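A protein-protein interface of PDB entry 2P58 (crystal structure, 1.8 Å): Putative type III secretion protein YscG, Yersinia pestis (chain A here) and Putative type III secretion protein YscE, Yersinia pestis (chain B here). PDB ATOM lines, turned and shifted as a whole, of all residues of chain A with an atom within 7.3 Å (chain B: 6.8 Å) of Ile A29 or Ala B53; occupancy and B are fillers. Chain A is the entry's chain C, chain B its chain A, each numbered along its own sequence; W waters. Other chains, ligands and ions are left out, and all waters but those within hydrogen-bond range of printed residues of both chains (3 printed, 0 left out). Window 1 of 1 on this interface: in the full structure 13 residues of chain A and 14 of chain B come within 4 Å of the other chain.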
ATOM      1  N   ASN A   7      -4.338  11.903  -7.754  1.00  0.00           N
ATOM      2  CA  ASN A   7      -4.908  11.516  -6.468  1.00  0.00           C
ATOM      3  C   ASN A   7      -4.118  10.440  -5.768  1.00  0.00           C
ATOM      4  O   ASN A   7      -4.109  10.378  -4.533  1.00  0.00           O
ATOM      5  CB  ASN A   7      -6.366  11.117  -6.633  1.00  0.00           C
ATOM      6  CG  ASN A   7      -7.250  12.316  -6.947  1.00  0.00           C
ATOM      7  OD1 ASN A   7      -6.935  13.456  -6.575  1.00  0.00           O
ATOM      8  ND2 ASN A   7      -8.361  12.068  -7.630  1.00  0.00           N
ATOM      9  N   LEU A   9      -0.837  10.217  -6.040  1.00  0.00           N
ATOM     10  CA  LEU A   9       0.308  10.960  -5.517  1.00  0.00           C
ATOM     11  C   LEU A   9      -0.081  11.650  -4.199  1.00  0.00           C
ATOM     12  O   LEU A   9       0.662  11.573  -3.228  1.00  0.00           O
ATOM     13  CB  LEU A   9       0.757  12.026  -6.513  1.00  0.00           C
ATOM     14  CG  LEU A   9       1.921  12.909  -6.091  1.00  0.00           C
ATOM     15  CD1 LEU A   9       3.170  12.069  -5.774  1.00  0.00           C
ATOM     16  CD2 LEU A   9       2.207  13.862  -7.262  1.00  0.00           C
ATOM     17  N   LEU A  10      -1.224  12.336  -4.192  1.00  0.00           N
ATOM     18  CA  LEU A  10      -1.700  13.024  -2.977  1.00  0.00           C
ATOM     19  C   LEU A  10      -1.907  12.022  -1.818  1.00  0.00           C
ATOM     20  O   LEU A  10      -1.525  12.287  -0.688  1.00  0.00           O
ATOM     21  CB  LEU A  10      -3.018  13.754  -3.229  1.00  0.00           C
ATOM     22  CG  LEU A  10      -2.845  14.949  -4.178  1.00  0.00           C
ATOM     23  CD1 LEU A  10      -4.231  15.520  -4.489  1.00  0.00           C
ATOM     24  CD2 LEU A  10      -1.980  16.005  -3.541  1.00  0.00           C
ATOM     25  N   ALA A  11      -2.507  10.874  -2.105  1.00  0.00           N
ATOM     26  CA  ALA A  11      -2.698   9.844  -1.056  1.00  0.00           C
ATOM     27  C   ALA A  11      -1.346   9.354  -0.495  1.00  0.00           C
ATOM     28  O   ALA A  11      -1.195   9.193   0.714  1.00  0.00           O
ATOM     29  CB  ALA A  11      -3.508   8.621  -1.616  1.00  0.00           C
ATOM     30  N   GLU A  12      -0.367   9.110  -1.358  1.00  0.00           N
ATOM     31  CA  GLU A  12       0.913   8.653  -0.873  1.00  0.00           C
ATOM     32  C   GLU A  12       1.587   9.747  -0.062  1.00  0.00           C
ATOM     33  O   GLU A  12       2.226   9.464   0.955  1.00  0.00           O
ATOM     34  CB  GLU A  12       1.806   8.222  -2.036  1.00  0.00           C
ATOM     35  CG  GLU A  12       1.361   6.902  -2.656  1.00  0.00           C
ATOM     36  CD  GLU A  12       2.427   6.263  -3.553  1.00  0.00           C
ATOM     37  OE1 GLU A  12       3.638   6.384  -3.268  1.00  0.00           O
ATOM     38  OE2 GLU A  12       2.046   5.606  -4.546  1.00  0.00           O
ATOM     39  N   ILE A  13       1.431  11.003  -0.490  1.00  0.00           N
ATOM     40  CA  ILE A  13       2.044  12.090   0.266  1.00  0.00           C
ATOM     41  C   ILE A  13       1.358  12.232   1.647  1.00  0.00           C
ATOM     42  O   ILE A  13       2.017  12.516   2.654  1.00  0.00           O
ATOM     43  CB  ILE A  13       1.996  13.428  -0.515  1.00  0.00           C
ATOM     44  CG1 ILE A  13       3.028  13.359  -1.649  1.00  0.00           C
ATOM     45  CG2 ILE A  13       2.446  14.589   0.389  1.00  0.00           C
ATOM     46  CD1 ILE A  13       2.952  14.483  -2.627  1.00  0.00           C
ATOM     47  N   ALA A  14       0.043  12.064   1.698  1.00  0.00           N
ATOM     48  CA  ALA A  14      -0.652  12.137   2.973  1.00  0.00           C
ATOM     49  C   ALA A  14      -0.103  11.062   3.910  1.00  0.00           C
ATOM     50  O   ALA A  14       0.070  11.301   5.103  1.00  0.00           O
ATOM     51  CB  ALA A  14      -2.169  11.921   2.770  1.00  0.00           C
ATOM     52  N   LEU A  15       0.165   9.874   3.367  1.00  0.00           N
ATOM     53  CA  LEU A  15       0.679   8.793   4.182  1.00  0.00           C
ATOM     54  C   LEU A  15       2.071   9.166   4.668  1.00  0.00           C
ATOM     55  O   LEU A  15       2.406   8.893   5.822  1.00  0.00           O
ATOM     56  CB  LEU A  15       0.687   7.467   3.416  1.00  0.00           C
ATOM     57  CG  LEU A  15      -0.716   6.873   3.199  1.00  0.00           C
ATOM     58  CD1 LEU A  15      -0.605   5.681   2.261  1.00  0.00           C
ATOM     59  CD2 LEU A  15      -1.365   6.470   4.544  1.00  0.00           C
ATOM     60  N   GLY A  17       2.932  12.079   5.225  1.00  0.00           N
ATOM     61  CA  GLY A  17       2.625  13.039   6.265  1.00  0.00           C
ATOM     62  C   GLY A  17       2.308  12.392   7.603  1.00  0.00           C
ATOM     63  O   GLY A  17       2.813  12.818   8.641  1.00  0.00           O
ATOM     64  N   HIS A  23       0.171  15.708  10.611  1.00  0.00           N
ATOM     65  CA  HIS A  23      -1.187  15.180  10.603  1.00  0.00           C
ATOM     66  C   HIS A  23      -2.278  16.073  10.029  1.00  0.00           C
ATOM     67  O   HIS A  23      -3.198  15.586   9.385  1.00  0.00           O
ATOM     68  CB  HIS A  23      -1.539  14.711  12.034  1.00  0.00           C
ATOM     69  CG  HIS A  23      -0.593  13.670  12.559  1.00  0.00           C
ATOM     70  ND1 HIS A  23      -0.573  12.375  12.082  1.00  0.00           N
ATOM     71  CD2 HIS A  23       0.427  13.757  13.447  1.00  0.00           C
ATOM     72  CE1 HIS A  23       0.423  11.711  12.648  1.00  0.00           C
ATOM     73  NE2 HIS A  23       1.047  12.530  13.481  1.00  0.00           N
ATOM     74  N   GLU A  24      -2.214  17.376  10.282  1.00  0.00           N
ATOM     75  CA  GLU A  24      -3.224  18.252   9.723  1.00  0.00           C
ATOM     76  C   GLU A  24      -3.062  18.370   8.216  1.00  0.00           C
ATOM     77  O   GLU A  24      -4.052  18.392   7.487  1.00  0.00           O
ATOM     78  CB  GLU A  24      -3.176  19.610  10.389  1.00  0.00           C
ATOM     79  CG  GLU A  24      -4.202  20.625   9.849  1.00  0.00           C
ATOM     80  CD  GLU A  24      -5.664  20.166   9.917  1.00  0.00           C
ATOM     81  OE1 GLU A  24      -6.066  19.444  10.874  1.00  0.00           O
ATOM     82  OE2 GLU A  24      -6.430  20.561   9.006  1.00  0.00           O
ATOM     83  N   GLU A  25      -1.825  18.361   7.728  1.00  0.00           N
ATOM     84  CA  GLU A  25      -1.618  18.418   6.280  1.00  0.00           C
ATOM     85  C   GLU A  25      -2.190  17.142   5.656  1.00  0.00           C
ATOM     86  O   GLU A  25      -2.834  17.177   4.615  1.00  0.00           O
ATOM     87  CB  GLU A  25      -0.119  18.512   5.957  1.00  0.00           C
ATOM     88  CG  GLU A  25       0.534  19.827   6.358  1.00  0.00           C
ATOM     89  CD  GLU A  25       0.859  19.995   7.850  1.00  0.00           C
ATOM     90  OE1 GLU A  25       0.650  19.070   8.693  1.00  0.00           O
ATOM     91  OE2 GLU A  25       1.369  21.099   8.172  1.00  0.00           O
ATOM     92  N   ALA A  26      -1.925  15.995   6.283  1.00  0.00           N
ATOM     93  CA  ALA A  26      -2.461  14.744   5.772  1.00  0.00           C
ATOM     94  C   ALA A  26      -4.001  14.761   5.797  1.00  0.00           C
ATOM     95  O   ALA A  26      -4.655  14.220   4.900  1.00  0.00           O
ATOM     96  CB  ALA A  26      -1.909  13.557   6.602  1.00  0.00           C
ATOM     97  N   ASN A  27      -4.592  15.387   6.814  1.00  0.00           N
ATOM     98  CA  ASN A  27      -6.046  15.432   6.912  1.00  0.00           C
ATOM     99  C   ASN A  27      -6.649  16.319   5.817  1.00  0.00           C
ATOM    100  O   ASN A  27      -7.721  16.020   5.283  1.00  0.00           O
ATOM    101  CB  ASN A  27      -6.477  15.966   8.280  1.00  0.00           C
ATOM    102  CG  ASN A  27      -7.973  15.838   8.485  1.00  0.00           C
ATOM    103  OD1 ASN A  27      -8.519  14.744   8.397  1.00  0.00           O
ATOM    104  ND2 ASN A  27      -8.636  16.950   8.747  1.00  0.00           N
ATOM    105  N   CYS A  28      -5.979  17.418   5.498  1.00  0.00           N
ATOM    106  CA  CYS A  28      -6.476  18.279   4.426  1.00  0.00           C
ATOM    107  C   CYS A  28      -6.481  17.498   3.137  1.00  0.00           C
ATOM    108  O   CYS A  28      -7.371  17.669   2.307  1.00  0.00           O
ATOM    109  CB  CYS A  28      -5.582  19.506   4.245  1.00  0.00           C
ATOM    110  SG  CYS A  28      -5.826  20.715   5.549  1.00  0.00           S
ATOM    111  N   ILE A  29      -5.465  16.664   2.928  1.00  0.00           N
ATOM    112  CA  ILE A  29      -5.469  15.874   1.706  1.00  0.00           C
ATOM    113  C   ILE A  29      -6.629  14.856   1.756  1.00  0.00           C
ATOM    114  O   ILE A  29      -7.341  14.623   0.762  1.00  0.00           O
ATOM    115  CB  ILE A  29      -4.136  15.123   1.516  1.00  0.00           C
ATOM    116  CG1 ILE A  29      -3.023  16.136   1.190  1.00  0.00           C
ATOM    117  CG2 ILE A  29      -4.286  14.081   0.406  1.00  0.00           C
ATOM    118  CD1 ILE A  29      -1.599  15.542   1.335  1.00  0.00           C
ATOM    119  N   ALA A  30      -6.803  14.223   2.911  1.00  0.00           N
ATOM    120  CA  ALA A  30      -7.914  13.266   3.043  1.00  0.00           C
ATOM    121  C   ALA A  30      -9.290  13.923   2.817  1.00  0.00           C
ATOM    122  O   ALA A  30     -10.204  13.265   2.298  1.00  0.00           O
ATOM    123  CB  ALA A  30      -7.863  12.564   4.422  1.00  0.00           C
ATOM    124  N   GLU A  31      -9.451  15.194   3.196  1.00  0.00           N
ATOM    125  CA  GLU A  31     -10.724  15.889   2.992  1.00  0.00           C
ATOM    126  C   GLU A  31     -10.998  15.979   1.491  1.00  0.00           C
ATOM    127  O   GLU A  31     -12.140  15.881   1.051  1.00  0.00           O
ATOM    128  CB  GLU A  31     -10.697  17.283   3.642  1.00  0.00           C
ATOM    129  CG  GLU A  31     -10.868  17.190   5.162  1.00  0.00           C
ATOM    130  CD  GLU A  31     -10.374  18.404   5.954  1.00  0.00           C
ATOM    131  OE1 GLU A  31     -10.939  18.633   7.043  1.00  0.00           O
ATOM    132  OE2 GLU A  31      -9.424  19.111   5.537  1.00  0.00           O
ATOM    133  N   TRP A  32      -9.946  16.147   0.709  1.00  0.00           N
ATOM    134  CA  TRP A  32     -10.093  16.176  -0.739  1.00  0.00           C
ATOM    135  C   TRP A  32     -10.442  14.771  -1.255  1.00  0.00           C
ATOM    136  O   TRP A  32     -11.352  14.606  -2.087  1.00  0.00           O
ATOM    137  CB  TRP A  32      -8.786  16.672  -1.404  1.00  0.00           C
ATOM    138  CG  TRP A  32      -8.736  16.425  -2.878  1.00  0.00           C
ATOM    139  CD1 TRP A  32      -7.832  15.642  -3.561  1.00  0.00           C
ATOM    140  CD2 TRP A  32      -9.609  16.975  -3.867  1.00  0.00           C
ATOM    141  NE1 TRP A  32      -8.101  15.687  -4.914  1.00  0.00           N
ATOM    142  CE2 TRP A  32      -9.183  16.500  -5.120  1.00  0.00           C
ATOM    143  CE3 TRP A  32     -10.711  17.838  -3.809  1.00  0.00           C
ATOM    144  CZ2 TRP A  32      -9.823  16.858  -6.313  1.00  0.00           C
ATOM    145  CZ3 TRP A  32     -11.336  18.192  -4.991  1.00  0.00           C
ATOM    146  CH2 TRP A  32     -10.892  17.706  -6.220  1.00  0.00           C
ATOM    147  N   LEU A  33      -9.701  13.763  -0.790  1.00  0.00           N
ATOM    148  CA  LEU A  33      -9.935  12.390  -1.234  1.00  0.00           C
ATOM    149  C   LEU A  33     -11.348  11.934  -0.863  1.00  0.00           C
ATOM    150  O   LEU A  33     -11.961  11.121  -1.575  1.00  0.00           O
ATOM    151  CB  LEU A  33      -8.877  11.445  -0.642  1.00  0.00           C
ATOM    152  CG  LEU A  33      -7.442  11.705  -1.130  1.00  0.00           C
ATOM    153  CD1 LEU A  33      -6.489  10.710  -0.472  1.00  0.00           C
ATOM    154  CD2 LEU A  33      -7.368  11.594  -2.653  1.00  0.00           C
ATOM    155  N   HIS A  34     -11.879  12.491   0.225  1.00  0.00           N
ATOM    156  CA  HIS A  34     -13.220  12.172   0.680  1.00  0.00           C
ATOM    157  C   HIS A  34     -14.248  12.759  -0.283  1.00  0.00           C
ATOM    158  O   HIS A  34     -15.248  12.122  -0.609  1.00  0.00           O
ATOM    159  CB  HIS A  34     -13.462  12.763   2.059  1.00  0.00           C
ATOM    160  CG  HIS A  34     -14.876  12.637   2.524  1.00  0.00           C
ATOM    161  ND1 HIS A  34     -15.467  11.415   2.758  1.00  0.00           N
ATOM    162  CD2 HIS A  34     -15.824  13.570   2.766  1.00  0.00           C
ATOM    163  CE1 HIS A  34     -16.725  11.600   3.126  1.00  0.00           C
ATOM    164  NE2 HIS A  34     -16.967  12.900   3.139  1.00  0.00           N
ATOM    165  N   LEU A  35     -14.017  13.993  -0.696  1.00  0.00           N
ATOM    166  CA  LEU A  35     -14.917  14.639  -1.623  1.00  0.00           C
ATOM    167  C   LEU A  35     -14.969  13.806  -2.898  1.00  0.00           C
ATOM    168  O   LEU A  35     -16.046  13.653  -3.496  1.00  0.00           O
ATOM    169  CB  LEU A  35     -14.405  16.059  -1.906  1.00  0.00           C
ATOM    170  CG  LEU A  35     -15.197  17.006  -2.788  1.00  0.00           C
ATOM    171  CD1 LEU A  35     -16.635  17.075  -2.320  1.00  0.00           C
ATOM    172  CD2 LEU A  35     -14.533  18.389  -2.682  1.00  0.00           C
ATOM    173  N   VAL A  42      -9.161   7.292   2.547  1.00  0.00           N
ATOM    174  CA  VAL A  42      -9.359   8.265   3.624  1.00  0.00           C
ATOM    175  C   VAL A  42      -9.227   7.528   4.969  1.00  0.00           C
ATOM    176  O   VAL A  42      -8.582   8.011   5.885  1.00  0.00           O
ATOM    177  CB  VAL A  42     -10.746   8.918   3.526  1.00  0.00           C
ATOM    178  CG1 VAL A  42     -11.073   9.700   4.766  1.00  0.00           C
ATOM    179  CG2 VAL A  42     -10.760   9.902   2.315  1.00  0.00           C
ATOM    180  N   ILE A  45      -5.588   6.660   5.739  1.00  0.00           N
ATOM    181  CA  ILE A  45      -4.839   7.837   6.224  1.00  0.00           C
ATOM    182  C   ILE A  45      -5.203   8.156   7.673  1.00  0.00           C
ATOM    183  O   ILE A  45      -4.332   8.446   8.483  1.00  0.00           O
ATOM    184  CB  ILE A  45      -5.112   9.105   5.312  1.00  0.00           C
ATOM    185  CG1 ILE A  45      -4.535   8.859   3.926  1.00  0.00           C
ATOM    186  CG2 ILE A  45      -4.540  10.369   5.956  1.00  0.00           C
ATOM    187  CD1 ILE A  45      -5.118   9.831   2.860  1.00  0.00           C
ATOM    188  N   LEU B  20       2.801  18.861  -8.641  1.00  0.00           N
ATOM    189  CA  LEU B  20       1.878  19.482  -7.695  1.00  0.00           C
ATOM    190  C   LEU B  20       1.800  20.990  -7.913  1.00  0.00           C
ATOM    191  O   LEU B  20       0.728  21.583  -7.859  1.00  0.00           O
ATOM    192  CB  LEU B  20       2.334  19.214  -6.262  1.00  0.00           C
ATOM    193  CG  LEU B  20       2.440  17.740  -5.844  1.00  0.00           C
ATOM    194  CD1 LEU B  20       3.253  17.670  -4.560  1.00  0.00           C
ATOM    195  CD2 LEU B  20       1.023  17.146  -5.666  1.00  0.00           C
ATOM    196  N   ARG B  45     -11.163  22.817  -1.595  1.00  0.00           N
ATOM    197  CA  ARG B  45     -10.691  21.548  -1.036  1.00  0.00           C
ATOM    198  C   ARG B  45      -9.475  21.058  -1.777  1.00  0.00           C
ATOM    199  O   ARG B  45      -8.521  20.549  -1.170  1.00  0.00           O
ATOM    200  CB  ARG B  45     -11.757  20.457  -1.170  1.00  0.00           C
ATOM    201  CG  ARG B  45     -12.112  19.802   0.133  1.00  0.00           C
ATOM    202  CD  ARG B  45     -12.917  20.785   0.948  1.00  0.00           C
ATOM    203  NE  ARG B  45     -14.074  20.129   1.562  1.00  0.00           N
ATOM    204  CZ  ARG B  45     -15.213  20.738   1.882  1.00  0.00           C
ATOM    205  NH1 ARG B  45     -15.390  22.038   1.650  1.00  0.00           N
ATOM    206  NH2 ARG B  45     -16.187  20.037   2.437  1.00  0.00           N
ATOM    207  N   LYS B  48      -6.375  23.336  -1.006  1.00  0.00           N
ATOM    208  CA  LYS B  48      -5.776  23.052   0.286  1.00  0.00           C
ATOM    209  C   LYS B  48      -5.023  21.713   0.278  1.00  0.00           C
ATOM    210  O   LYS B  48      -3.962  21.573   0.914  1.00  0.00           O
ATOM    211  CB  LYS B  48      -6.839  23.048   1.379  1.00  0.00           C
ATOM    212  CG  LYS B  48      -6.215  23.178   2.767  1.00  0.00           C
ATOM    213  CD  LYS B  48      -5.427  24.504   2.849  1.00  0.00           C
ATOM    214  CE  LYS B  48      -4.609  24.607   4.132  1.00  0.00           C
ATOM    215  NZ  LYS B  48      -5.474  24.383   5.313  1.00  0.00           N
ATOM    216  N   ALA B  49      -5.561  20.728  -0.432  1.00  0.00           N
ATOM    217  CA  ALA B  49      -4.899  19.422  -0.509  1.00  0.00           C
ATOM    218  C   ALA B  49      -3.543  19.561  -1.222  1.00  0.00           C
ATOM    219  O   ALA B  49      -2.517  18.993  -0.812  1.00  0.00           O
ATOM    220  CB  ALA B  49      -5.780  18.445  -1.246  1.00  0.00           C
ATOM    221  N   LEU B  50      -3.535  20.341  -2.293  1.00  0.00           N
ATOM    222  CA  LEU B  50      -2.286  20.518  -3.035  1.00  0.00           C
ATOM    223  C   LEU B  50      -1.267  21.274  -2.207  1.00  0.00           C
ATOM    224  O   LEU B  50      -0.097  20.892  -2.184  1.00  0.00           O
ATOM    225  CB  LEU B  50      -2.556  21.268  -4.347  1.00  0.00           C
ATOM    226  CG  LEU B  50      -3.256  20.430  -5.417  1.00  0.00           C
ATOM    227  CD1 LEU B  50      -3.781  21.344  -6.516  1.00  0.00           C
ATOM    228  CD2 LEU B  50      -2.288  19.381  -5.982  1.00  0.00           C
ATOM    229  N   GLU B  51      -1.695  22.354  -1.540  1.00  0.00           N
ATOM    230  CA  GLU B  51      -0.787  23.145  -0.724  1.00  0.00           C
ATOM    231  C   GLU B  51      -0.208  22.251   0.361  1.00  0.00           C
ATOM    232  O   GLU B  51       0.972  22.322   0.680  1.00  0.00           O
ATOM    233  CB  GLU B  51      -1.533  24.335  -0.083  1.00  0.00           C
ATOM    234  CG  GLU B  51      -1.926  25.401  -1.118  1.00  0.00           C
ATOM    235  CD  GLU B  51      -2.953  26.406  -0.587  1.00  0.00           C
ATOM    236  OE1 GLU B  51      -3.345  26.299   0.604  1.00  0.00           O
ATOM    237  OE2 GLU B  51      -3.374  27.296  -1.375  1.00  0.00           O
ATOM    238  N   SER B  52      -1.066  21.415   0.931  1.00  0.00           N
ATOM    239  CA  SER B  52      -0.644  20.505   2.006  1.00  0.00           C
ATOM    240  C   SER B  52       0.379  19.489   1.536  1.00  0.00           C
ATOM    241  O   SER B  52       1.307  19.140   2.255  1.00  0.00           O
ATOM    242  CB  SER B  52      -1.877  19.781   2.555  1.00  0.00           C
ATOM    243  OG  SER B  52      -2.714  20.712   3.243  1.00  0.00           O
ATOM    244  N   ALA B  53       0.155  18.946   0.350  1.00  0.00           N
ATOM    245  CA  ALA B  53       1.072  17.976  -0.205  1.00  0.00           C
ATOM    246  C   ALA B  53       2.430  18.617  -0.494  1.00  0.00           C
ATOM    247  O   ALA B  53       3.478  18.055  -0.199  1.00  0.00           O
ATOM    248  CB  ALA B  53       0.472  17.379  -1.506  1.00  0.00           C
ATOM    249  N   ILE B  54       2.408  19.811  -1.072  1.00  0.00           N
ATOM    250  CA  ILE B  54       3.666  20.503  -1.378  1.00  0.00           C
ATOM    251  C   ILE B  54       4.436  20.737  -0.077  1.00  0.00           C
ATOM    252  O   ILE B  54       5.648  20.515  -0.014  1.00  0.00           O
ATOM    253  CB  ILE B  54       3.360  21.857  -2.104  1.00  0.00           C
ATOM    254  CG1 ILE B  54       2.815  21.566  -3.500  1.00  0.00           C
ATOM    255  CG2 ILE B  54       4.593  22.736  -2.143  1.00  0.00           C
ATOM    256  CD1 ILE B  54       2.032  22.737  -4.127  1.00  0.00           C
ATOM    257  N   ALA B  55       3.715  21.137   0.969  1.00  0.00           N
ATOM    258  CA  ALA B  55       4.309  21.381   2.278  1.00  0.00           C
ATOM    259  C   ALA B  55       4.975  20.118   2.817  1.00  0.00           C
ATOM    260  O   ALA B  55       6.138  20.151   3.201  1.00  0.00           O
ATOM    261  CB  ALA B  55       3.255  21.868   3.250  1.00  0.00           C
ATOM    262  N   ILE B  56       4.242  18.999   2.829  1.00  0.00           N
ATOM    263  CA  ILE B  56       4.826  17.751   3.341  1.00  0.00           C
ATOM    264  C   ILE B  56       6.084  17.392   2.576  1.00  0.00           C
ATOM    265  O   ILE B  56       7.110  17.020   3.177  1.00  0.00           O
ATOM    266  CB  ILE B  56       3.830  16.574   3.229  1.00  0.00           C
ATOM    267  CG1 ILE B  56       2.732  16.761   4.257  1.00  0.00           C
ATOM    268  CG2 ILE B  56       4.558  15.208   3.494  1.00  0.00           C
ATOM    269  CD1 ILE B  56       1.518  15.876   3.989  1.00  0.00           C
ATOM    270  N   ILE B  57       6.038  17.515   1.256  1.00  0.00           N
ATOM    271  CA  ILE B  57       7.231  17.169   0.466  1.00  0.00           C
ATOM    272  C   ILE B  57       8.380  18.103   0.838  1.00  0.00           C
ATOM    273  O   ILE B  57       9.520  17.659   0.967  1.00  0.00           O
ATOM    274  CB  ILE B  57       6.947  17.249  -1.047  1.00  0.00           C
ATOM    275  CG1 ILE B  57       6.012  16.100  -1.463  1.00  0.00           C
ATOM    276  CG2 ILE B  57       8.277  17.177  -1.838  1.00  0.00           C
ATOM    277  CD1 ILE B  57       6.587  14.690  -1.205  1.00  0.00           C
ATOM    278  N   HIS B  58       8.102  19.393   1.019  1.00  0.00           N
ATOM    279  CA  HIS B  58       9.183  20.317   1.411  1.00  0.00           C
ATOM    280  C   HIS B  58       9.781  19.927   2.760  1.00  0.00           C
ATOM    281  O   HIS B  58      10.999  19.850   2.941  1.00  0.00           O
ATOM    282  CB  HIS B  58       8.658  21.755   1.535  1.00  0.00           C
ATOM    283  CG  HIS B  58       8.398  22.416   0.220  1.00  0.00           C
ATOM    284  ND1 HIS B  58       7.961  23.723   0.118  1.00  0.00           N
ATOM    285  CD2 HIS B  58       8.546  21.965  -1.050  1.00  0.00           C
ATOM    286  CE1 HIS B  58       7.858  24.048  -1.162  1.00  0.00           C
ATOM    287  NE2 HIS B  58       8.205  22.999  -1.888  1.00  0.00           N
HETATM  288  O   HOH W   1     -14.416  17.203   2.062  1.00  0.00           O
HETATM  289  O   HOH W   2     -12.268  20.648   4.481  1.00  0.00           O
HETATM  290  O   HOH W   3      -8.800  19.866   1.505  1.00  0.00           O
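The side-chain hydroxyl (OG) of Ser B52 sits at hydrogen-bond distance from the backbone carbonyl oxygen (O) of Lys B48, 2.8 Å away.
The indole nitrogen (NE1) of Trp A32 lies within hydrogen-bond range of the side-chain amide oxygen (OD1) of Asn A7 (3.0 Å).
The backbone carbonyl oxygen (O) of Glu A24 lies within hydrogen-bond range of the side-chain sulfur (SG) of Cys A28 (3.5 Å).
The side-chain amino group (NZ) of Lys B48 lies within hydrogen-bond range of the side-chain sulfur (SG) of Cys A28.
Of the printed residues of chain B, Leu A10 touches Leu B20 (3.9 Å) and Ala B53 (3.5 Å).
Of chain B, only Ala B49 (3.5 Å) and Ala B53 (3.9 Å) come within 4 Å of Ile A29.
Of the printed residues of chain A, Arg B45 touches Trp A32 and Leu A35.
Ala B53 touches just these residues of chain A: Leu A10 (3.5 Å), Ile A13 (3.7 Å) and Ile A29 (3.9 Å).
The nearest printed residue of chain A that does not touch Ser B52 is Ile A29 (4.1 Å).
Of the 24 printed residues of chain A, 9 touch a printed residue of chain B.
Hydrophobic or aromatic side chains of chain A within 4 Å of the printed part of chain B: Leu A9, Leu A10, Ile A13, Ile A29, Trp A32 and Leu A35.
Along chain A the printed residues that touch a printed residue of chain B span positions 9 to 35.
Printed residues of chain B that touch a printed residue of chain A: Leu B20, Arg B45, Lys B48, Ala B49, Ser B52, Ala B53, Ile B56 and Ile B57.
Hydrophobic or aromatic side chains of chain B within 4 Å of the printed part of chain A: Leu B20, Ala B49, Ala B53, Ile B56 and Ile B57.
Along chain B the printed residues that touch a printed residue of chain A span positions 20 to 57.
Water W3 bridges the backbone carbonyl oxygen (O) of Cys A28 and the backbone carbonyl oxygen (O) of Arg B45.
Water W1 lies within hydrogen-bond range of the backbone carbonyl oxygen of Glu A31 (2.8 Å) and the guanidinium group of Arg B45 (3.0 Å).
Water W2 bridges OE2 of Glu A31 and NE of Arg B45.
Leu B20 touches Leu A9 (CD2 to CD2, 3.8 Å).
Ala B53 touches Leu A10.
Leu B20 touches Ile A13.
Ile A13 touches Ile B57 (CD1 to CG1, 3.7 Å).
Ile B56 touches Gly A17.
CB of Ser B52 touches O of Glu A25, 3.5 Å away.
Cys A28 touches Ala B49.
CB of Cys A28 touches OG of Ser B52, at 3.3 Å.
CD1 of Ile A29 touches CA of Ala B53, 3.9 Å away.
CB of Ala B49 touches CB of Trp A32 (3.5 Å).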
